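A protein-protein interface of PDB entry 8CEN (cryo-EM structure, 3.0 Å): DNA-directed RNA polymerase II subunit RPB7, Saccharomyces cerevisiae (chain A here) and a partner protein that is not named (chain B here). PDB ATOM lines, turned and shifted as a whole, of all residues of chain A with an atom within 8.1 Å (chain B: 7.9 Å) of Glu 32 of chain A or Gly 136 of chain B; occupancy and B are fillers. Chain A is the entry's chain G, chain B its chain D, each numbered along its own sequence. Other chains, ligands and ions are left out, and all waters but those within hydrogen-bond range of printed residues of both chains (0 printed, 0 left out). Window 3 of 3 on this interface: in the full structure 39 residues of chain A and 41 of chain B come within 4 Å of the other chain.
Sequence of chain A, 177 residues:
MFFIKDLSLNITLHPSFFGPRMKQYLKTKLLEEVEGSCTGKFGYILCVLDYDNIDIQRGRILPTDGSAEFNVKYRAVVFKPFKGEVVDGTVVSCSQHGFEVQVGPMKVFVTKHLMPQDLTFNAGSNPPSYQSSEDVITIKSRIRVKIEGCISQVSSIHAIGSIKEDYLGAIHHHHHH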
ATOM      1  N   ILE A  11     -19.900  18.146  24.694  1.00  0.00           N
ATOM      2  CA  ILE A  11     -19.333  18.254  23.356  1.00  0.00           C
ATOM      3  C   ILE A  11     -20.403  18.811  22.424  1.00  0.00           C
ATOM      4  O   ILE A  11     -21.597  18.529  22.586  1.00  0.00           O
ATOM      5  CB  ILE A  11     -18.783  16.894  22.870  1.00  0.00           C
ATOM      6  CG1 ILE A  11     -18.056  17.027  21.527  1.00  0.00           C
ATOM      7  CG2 ILE A  11     -19.879  15.850  22.782  1.00  0.00           C
ATOM      8  CD1 ILE A  11     -16.829  17.905  21.588  1.00  0.00           C
ATOM      9  N   GLN A  24     -20.962   7.591  15.912  1.00  0.00           N
ATOM     10  CA  GLN A  24     -19.573   7.425  15.494  1.00  0.00           C
ATOM     11  C   GLN A  24     -18.861   8.772  15.400  1.00  0.00           C
ATOM     12  O   GLN A  24     -17.701   8.898  15.816  1.00  0.00           O
ATOM     13  CB  GLN A  24     -19.513   6.676  14.159  1.00  0.00           C
ATOM     14  CG  GLN A  24     -18.277   6.966  13.316  1.00  0.00           C
ATOM     15  CD  GLN A  24     -18.201   6.116  12.064  1.00  0.00           C
ATOM     16  OE1 GLN A  24     -18.996   6.279  11.139  1.00  0.00           O
ATOM     17  NE2 GLN A  24     -17.236   5.204  12.025  1.00  0.00           N
ATOM     18  N   TYR A  25     -19.547   9.792  14.873  1.00  0.00           N
ATOM     19  CA  TYR A  25     -18.965  11.133  14.834  1.00  0.00           C
ATOM     20  C   TYR A  25     -18.735  11.683  16.239  1.00  0.00           C
ATOM     21  O   TYR A  25     -17.728  12.358  16.495  1.00  0.00           O
ATOM     22  CB  TYR A  25     -19.857  12.074  14.027  1.00  0.00           C
ATOM     23  CG  TYR A  25     -19.977  11.715  12.562  1.00  0.00           C
ATOM     24  CD1 TYR A  25     -18.956  11.037  11.906  1.00  0.00           C
ATOM     25  CD2 TYR A  25     -21.107  12.062  11.836  1.00  0.00           C
ATOM     26  CE1 TYR A  25     -19.062  10.713  10.567  1.00  0.00           C
ATOM     27  CE2 TYR A  25     -21.223  11.741  10.497  1.00  0.00           C
ATOM     28  CZ  TYR A  25     -20.197  11.068   9.867  1.00  0.00           C
ATOM     29  OH  TYR A  25     -20.310  10.748   8.535  1.00  0.00           O
ATOM     30  N   LEU A  26     -19.659  11.397  17.161  1.00  0.00           N
ATOM     31  CA  LEU A  26     -19.493  11.788  18.557  1.00  0.00           C
ATOM     32  C   LEU A  26     -18.273  11.126  19.178  1.00  0.00           C
ATOM     33  O   LEU A  26     -17.499  11.780  19.885  1.00  0.00           O
ATOM     34  CB  LEU A  26     -20.742  11.422  19.355  1.00  0.00           C
ATOM     35  CG  LEU A  26     -21.875  12.439  19.362  1.00  0.00           C
ATOM     36  CD1 LEU A  26     -23.153  11.812  19.885  1.00  0.00           C
ATOM     37  CD2 LEU A  26     -21.471  13.637  20.198  1.00  0.00           C
ATOM     38  N   LYS A  27     -18.086   9.830  18.924  1.00  0.00           N
ATOM     39  CA  LYS A  27     -16.941   9.123  19.487  1.00  0.00           C
ATOM     40  C   LYS A  27     -15.627   9.616  18.887  1.00  0.00           C
ATOM     41  O   LYS A  27     -14.625   9.738  19.601  1.00  0.00           O
ATOM     42  CB  LYS A  27     -17.104   7.616  19.291  1.00  0.00           C
ATOM     43  CG  LYS A  27     -18.229   7.025  20.125  1.00  0.00           C
ATOM     44  CD  LYS A  27     -18.143   5.512  20.217  1.00  0.00           C
ATOM     45  CE  LYS A  27     -19.120   4.850  19.262  1.00  0.00           C
ATOM     46  NZ  LYS A  27     -18.790   3.418  19.038  1.00  0.00           N
ATOM     47  N   THR A  28     -15.614   9.929  17.589  1.00  0.00           N
ATOM     48  CA  THR A  28     -14.384  10.434  16.979  1.00  0.00           C
ATOM     49  C   THR A  28     -14.041  11.834  17.482  1.00  0.00           C
ATOM     50  O   THR A  28     -12.867  12.138  17.725  1.00  0.00           O
ATOM     51  CB  THR A  28     -14.491  10.422  15.455  1.00  0.00           C
ATOM     52  OG1 THR A  28     -15.708  11.057  15.048  1.00  0.00           O
ATOM     53  CG2 THR A  28     -14.456   8.994  14.925  1.00  0.00           C
ATOM     54  N   LYS A  29     -15.038  12.707  17.644  1.00  0.00           N
ATOM     55  CA  LYS A  29     -14.729  14.009  18.227  1.00  0.00           C
ATOM     56  C   LYS A  29     -14.376  13.895  19.702  1.00  0.00           C
ATOM     57  O   LYS A  29     -13.572  14.688  20.199  1.00  0.00           O
ATOM     58  CB  LYS A  29     -15.873  14.993  18.008  1.00  0.00           C
ATOM     59  CG  LYS A  29     -16.041  15.352  16.550  1.00  0.00           C
ATOM     60  CD  LYS A  29     -17.131  16.368  16.342  1.00  0.00           C
ATOM     61  CE  LYS A  29     -17.311  16.634  14.867  1.00  0.00           C
ATOM     62  NZ  LYS A  29     -16.124  17.322  14.290  1.00  0.00           N
ATOM     63  N   LEU A  30     -14.911  12.890  20.399  1.00  0.00           N
ATOM     64  CA  LEU A  30     -14.447  12.596  21.749  1.00  0.00           C
ATOM     65  C   LEU A  30     -12.967  12.231  21.741  1.00  0.00           C
ATOM     66  O   LEU A  30     -12.196  12.727  22.569  1.00  0.00           O
ATOM     67  CB  LEU A  30     -15.281  11.462  22.344  1.00  0.00           C
ATOM     68  CG  LEU A  30     -15.014  11.031  23.784  1.00  0.00           C
ATOM     69  CD1 LEU A  30     -15.311  12.179  24.730  1.00  0.00           C
ATOM     70  CD2 LEU A  30     -15.848   9.818  24.137  1.00  0.00           C
ATOM     71  N   LEU A  31     -12.547  11.415  20.768  1.00  0.00           N
ATOM     72  CA  LEU A  31     -11.140  11.038  20.649  1.00  0.00           C
ATOM     73  C   LEU A  31     -10.254  12.253  20.382  1.00  0.00           C
ATOM     74  O   LEU A  31      -9.442  12.640  21.228  1.00  0.00           O
ATOM     75  CB  LEU A  31     -10.968   9.992  19.547  1.00  0.00           C
ATOM     76  CG  LEU A  31     -11.577   8.618  19.830  1.00  0.00           C
ATOM     77  CD1 LEU A  31     -11.172   7.616  18.761  1.00  0.00           C
ATOM     78  CD2 LEU A  31     -11.185   8.127  21.215  1.00  0.00           C
ATOM     79  N   GLU A  32     -10.417  12.895  19.225  1.00  0.00           N
ATOM     80  CA  GLU A  32      -9.567  14.055  18.931  1.00  0.00           C
ATOM     81  C   GLU A  32      -9.996  15.357  19.611  1.00  0.00           C
ATOM     82  O   GLU A  32      -9.586  16.427  19.150  1.00  0.00           O
ATOM     83  CB  GLU A  32      -9.391  14.292  17.417  1.00  0.00           C
ATOM     84  CG  GLU A  32      -8.608  13.209  16.623  1.00  0.00           C
ATOM     85  CD  GLU A  32      -9.272  11.859  16.483  1.00  0.00           C
ATOM     86  OE1 GLU A  32      -8.542  10.858  16.317  1.00  0.00           O
ATOM     87  OE2 GLU A  32     -10.507  11.797  16.461  1.00  0.00           O
ATOM     88  N   GLU A  33     -10.797  15.316  20.680  1.00  0.00           N
ATOM     89  CA  GLU A  33     -10.878  16.447  21.595  1.00  0.00           C
ATOM     90  C   GLU A  33     -10.529  16.105  23.038  1.00  0.00           C
ATOM     91  O   GLU A  33     -10.432  17.022  23.862  1.00  0.00           O
ATOM     92  CB  GLU A  33     -12.277  17.081  21.551  1.00  0.00           C
ATOM     93  CG  GLU A  33     -12.612  17.736  20.221  1.00  0.00           C
ATOM     94  CD  GLU A  33     -11.755  18.950  19.933  1.00  0.00           C
ATOM     95  OE1 GLU A  33     -11.359  19.644  20.893  1.00  0.00           O
ATOM     96  OE2 GLU A  33     -11.470  19.205  18.746  1.00  0.00           O
ATOM     97  N   VAL A  34     -10.338  14.826  23.375  1.00  0.00           N
ATOM     98  CA  VAL A  34     -10.002  14.419  24.730  1.00  0.00           C
ATOM     99  C   VAL A  34      -8.626  13.769  24.811  1.00  0.00           C
ATOM    100  O   VAL A  34      -7.857  14.054  25.737  1.00  0.00           O
ATOM    101  CB  VAL A  34     -11.092  13.485  25.304  1.00  0.00           C
ATOM    102  CG1 VAL A  34     -10.714  12.966  26.661  1.00  0.00           C
ATOM    103  CG2 VAL A  34     -12.389  14.247  25.428  1.00  0.00           C
ATOM    104  N   GLU A  35      -8.285  12.908  23.849  1.00  0.00           N
ATOM    105  CA  GLU A  35      -6.994  12.230  23.847  1.00  0.00           C
ATOM    106  C   GLU A  35      -5.855  13.228  23.688  1.00  0.00           C
ATOM    107  O   GLU A  35      -5.755  13.914  22.666  1.00  0.00           O
ATOM    108  CB  GLU A  35      -6.952  11.209  22.716  1.00  0.00           C
ATOM    109  CG  GLU A  35      -7.719   9.943  22.996  1.00  0.00           C
ATOM    110  CD  GLU A  35      -7.442   8.874  21.969  1.00  0.00           C
ATOM    111  OE1 GLU A  35      -7.998   7.771  22.103  1.00  0.00           O
ATOM    112  OE2 GLU A  35      -6.666   9.138  21.027  1.00  0.00           O
ATOM    113  N   GLY A  36      -5.002  13.311  24.704  1.00  0.00           N
ATOM    114  CA  GLY A  36      -3.915  14.264  24.714  1.00  0.00           C
ATOM    115  C   GLY A  36      -4.305  15.663  25.124  1.00  0.00           C
ATOM    116  O   GLY A  36      -3.425  16.528  25.227  1.00  0.00           O
ATOM    117  N   SER A  37      -5.588  15.917  25.365  1.00  0.00           N
ATOM    118  CA  SER A  37      -6.034  17.227  25.808  1.00  0.00           C
ATOM    119  C   SER A  37      -5.678  17.429  27.271  1.00  0.00           C
ATOM    120  O   SER A  37      -5.761  16.501  28.080  1.00  0.00           O
ATOM    121  CB  SER A  37      -7.541  17.379  25.615  1.00  0.00           C
ATOM    122  OG  SER A  37      -8.249  16.584  26.548  1.00  0.00           O
ATOM    123  N   VAL A  48      -8.738   7.070  26.200  1.00  0.00           N
ATOM    124  CA  VAL A  48     -10.118   6.835  26.608  1.00  0.00           C
ATOM    125  C   VAL A  48     -10.342   5.332  26.730  1.00  0.00           C
ATOM    126  O   VAL A  48     -10.193   4.591  25.751  1.00  0.00           O
ATOM    127  CB  VAL A  48     -11.105   7.461  25.614  1.00  0.00           C
ATOM    128  CG1 VAL A  48     -12.525   7.020  25.926  1.00  0.00           C
ATOM    129  CG2 VAL A  48     -10.993   8.976  25.646  1.00  0.00           C
ATOM    130  N   TYR A  51     -14.010   2.008  24.920  1.00  0.00           N
ATOM    131  CA  TYR A  51     -14.516   2.672  23.726  1.00  0.00           C
ATOM    132  C   TYR A  51     -15.750   1.984  23.157  1.00  0.00           C
ATOM    133  O   TYR A  51     -16.542   2.633  22.466  1.00  0.00           O
ATOM    134  CB  TYR A  51     -13.408   2.740  22.670  1.00  0.00           C
ATOM    135  CG  TYR A  51     -13.763   3.507  21.415  1.00  0.00           C
ATOM    136  CD1 TYR A  51     -13.636   4.889  21.366  1.00  0.00           C
ATOM    137  CD2 TYR A  51     -14.195   2.846  20.271  1.00  0.00           C
ATOM    138  CE1 TYR A  51     -13.950   5.594  20.219  1.00  0.00           C
ATOM    139  CE2 TYR A  51     -14.512   3.542  19.120  1.00  0.00           C
ATOM    140  CZ  TYR A  51     -14.385   4.916  19.099  1.00  0.00           C
ATOM    141  OH  TYR A  51     -14.698   5.613  17.956  1.00  0.00           O
ATOM    142  N   LEU B 130       0.080   3.117  17.735  1.00  0.00           N
ATOM    143  CA  LEU B 130      -0.425   4.465  17.967  1.00  0.00           C
ATOM    144  C   LEU B 130      -0.912   5.099  16.671  1.00  0.00           C
ATOM    145  O   LEU B 130      -2.045   5.596  16.591  1.00  0.00           O
ATOM    146  CB  LEU B 130       0.688   5.305  18.598  1.00  0.00           C
ATOM    147  CG  LEU B 130       0.463   6.752  19.030  1.00  0.00           C
ATOM    148  CD1 LEU B 130      -0.577   6.803  20.122  1.00  0.00           C
ATOM    149  CD2 LEU B 130       1.766   7.380  19.497  1.00  0.00           C
ATOM    150  N   GLU B 131      -0.073   5.061  15.630  1.00  0.00           N
ATOM    151  CA  GLU B 131      -0.436   5.691  14.363  1.00  0.00           C
ATOM    152  C   GLU B 131      -1.559   4.942  13.655  1.00  0.00           C
ATOM    153  O   GLU B 131      -2.320   5.550  12.893  1.00  0.00           O
ATOM    154  CB  GLU B 131       0.789   5.797  13.455  1.00  0.00           C
ATOM    155  CG  GLU B 131       1.871   6.738  13.971  1.00  0.00           C
ATOM    156  CD  GLU B 131       1.430   8.191  13.994  1.00  0.00           C
ATOM    157  OE1 GLU B 131       0.621   8.587  13.129  1.00  0.00           O
ATOM    158  OE2 GLU B 131       1.900   8.943  14.875  1.00  0.00           O
ATOM    159  N   THR B 133      -4.037   3.306  15.363  1.00  0.00           N
ATOM    160  CA  THR B 133      -5.259   3.425  16.149  1.00  0.00           C
ATOM    161  C   THR B 133      -5.803   4.848  16.137  1.00  0.00           C
ATOM    162  O   THR B 133      -6.930   5.086  15.690  1.00  0.00           O
ATOM    163  CB  THR B 133      -5.004   2.968  17.587  1.00  0.00           C
ATOM    164  OG1 THR B 133      -4.578   1.599  17.587  1.00  0.00           O
ATOM    165  CG2 THR B 133      -6.266   3.105  18.421  1.00  0.00           C
ATOM    166  N   THR B 134      -5.021   5.807  16.616  1.00  0.00           N
ATOM    167  CA  THR B 134      -5.546   7.143  16.849  1.00  0.00           C
ATOM    168  C   THR B 134      -5.035   8.131  15.805  1.00  0.00           C
ATOM    169  O   THR B 134      -4.024   7.903  15.135  1.00  0.00           O
ATOM    170  CB  THR B 134      -5.205   7.622  18.262  1.00  0.00           C
ATOM    171  OG1 THR B 134      -5.741   8.934  18.476  1.00  0.00           O
ATOM    172  CG2 THR B 134      -3.720   7.623  18.476  1.00  0.00           C
ATOM    173  N   GLY B 135      -5.765   9.238  15.676  1.00  0.00           N
ATOM    174  CA  GLY B 135      -5.551  10.196  14.610  1.00  0.00           C
ATOM    175  C   GLY B 135      -4.666  11.372  14.965  1.00  0.00           C
ATOM    176  O   GLY B 135      -3.436  11.263  14.925  1.00  0.00           O
ATOM    177  N   GLY B 136      -5.281  12.520  15.275  1.00  0.00           N
ATOM    178  CA  GLY B 136      -4.530  13.731  15.530  1.00  0.00           C
ATOM    179  C   GLY B 136      -4.282  14.006  17.008  1.00  0.00           C
ATOM    180  O   GLY B 136      -4.878  13.379  17.883  1.00  0.00           O
ATOM    181  N   ASN B 137      -3.385  14.972  17.246  1.00  0.00           N
ATOM    182  CA  ASN B 137      -3.041  15.491  18.574  1.00  0.00           C
ATOM    183  C   ASN B 137      -2.555  14.384  19.513  1.00  0.00           C
ATOM    184  O   ASN B 137      -3.071  14.195  20.618  1.00  0.00           O
ATOM    185  CB  ASN B 137      -4.216  16.256  19.193  1.00  0.00           C
ATOM    186  CG  ASN B 137      -3.773  17.231  20.268  1.00  0.00           C
ATOM    187  OD1 ASN B 137      -2.585  17.339  20.572  1.00  0.00           O
ATOM    188  ND2 ASN B 137      -4.731  17.938  20.859  1.00  0.00           N
ATOM    189  N   ASN B 138      -1.539  13.655  19.058  1.00  0.00           N
ATOM    190  CA  ASN B 138      -0.976  12.557  19.831  1.00  0.00           C
ATOM    191  C   ASN B 138       0.465  12.797  20.253  1.00  0.00           C
ATOM    192  O   ASN B 138       1.188  11.830  20.514  1.00  0.00           O
ATOM    193  CB  ASN B 138      -1.090  11.250  19.053  1.00  0.00           C
ATOM    194  CG  ASN B 138      -2.526  10.858  18.815  1.00  0.00           C
ATOM    195  OD1 ASN B 138      -2.995  10.821  17.684  1.00  0.00           O
ATOM    196  ND2 ASN B 138      -3.251  10.592  19.898  1.00  0.00           N
ATOM    197  N   LYS B 139       0.904  14.056  20.312  1.00  0.00           N
ATOM    198  CA  LYS B 139       2.212  14.357  20.880  1.00  0.00           C
ATOM    199  C   LYS B 139       2.281  13.929  22.340  1.00  0.00           C
ATOM    200  O   LYS B 139       3.208  13.217  22.746  1.00  0.00           O
ATOM    201  CB  LYS B 139       2.509  15.850  20.744  1.00  0.00           C
ATOM    202  CG  LYS B 139       3.871  16.266  21.275  1.00  0.00           C
ATOM    203  CD  LYS B 139       5.014  15.629  20.504  1.00  0.00           C
ATOM    204  CE  LYS B 139       5.115  16.197  19.100  1.00  0.00           C
ATOM    205  NZ  LYS B 139       6.268  15.629  18.353  1.00  0.00           N
ATOM    206  N   LEU B 141       0.315  11.824  24.013  1.00  0.00           N
ATOM    207  CA  LEU B 141       0.169  10.381  24.166  1.00  0.00           C
ATOM    208  C   LEU B 141       1.419   9.637  23.711  1.00  0.00           C
ATOM    209  O   LEU B 141       1.783   8.617  24.309  1.00  0.00           O
ATOM    210  CB  LEU B 141      -1.066   9.897  23.403  1.00  0.00           C
ATOM    211  CG  LEU B 141      -1.463   8.429  23.562  1.00  0.00           C
ATOM    212  CD1 LEU B 141      -1.656   8.091  25.029  1.00  0.00           C
ATOM    213  CD2 LEU B 141      -2.741   8.154  22.791  1.00  0.00           C
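O of Asn 137 of chain B sits close to O of Glu 35 of chain A (3.4 Å). The side-chain carboxylate (OE2) of Glu 35 of chain A sits at hydrogen-bond distance from the side-chain hydroxyl (OG1) of Thr 134 of chain B (2.7 Å). The side-chain carboxylate (OE1) of Glu 32 of chain A lies within hydrogen-bond range of the backbone NH (N) of Gly 135 of chain B (3.3 Å).
O of Gly 136 of chain B lies close to OD1 of Asn 138 of chain B (3.2 Å). The backbone carbonyl oxygen (O) of Gly 135 of chain B sits close to the side-chain amide oxygen (OD1) of Asn 138 of chain B, 2.8 Å away. The backbone carbonyl oxygen (O) of Thr 28 of chain A lies close to the side-chain carboxylate (OE2) of Glu 32 of chain A (2.7 Å). OG1 of Thr 134 of chain B sits at hydrogen-bond distance from ND2 of Asn 138 of chain B, at 3.3 Å.
Glu 32 of chain A touches two residues of chain B. Of the printed residues of chain A, Gly 136 of chain B touches Glu 32 (3.7 Å). Printed residues of chain A within 4 Å of Thr 134 of chain B: Glu 35. Printed residues of chain A within 4 Å of Asn 137 of chain B: Glu 35. Lys 27 of chain A touches none of the printed residues of chain B. Ile 11 of chain A touches none of the printed residues of chain B. The nearest residue of chain A that does not touch Gly 136 of chain B is Glu 35 of chain A (4.9 Å). The nearest printed residue of chain A that does not touch Thr 134 of chain B is Glu 32 of chain A (4.03 Å).
Of the 17 printed residues of chain A, 2 touch a printed residue of chain B. Along chain B the printed residues that touch a printed residue of chain A span positions 134 to 138. Among the printed residues, no Asp or Glu carboxylate lies within 4 Å of a Lys or Arg side-chain nitrogen of the other chain.
Glu 32 of chain A touches Gly 136 of chain B (CG to N, 3.7 Å). Glu 35 of chain A touches Asn 138 of chain B.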
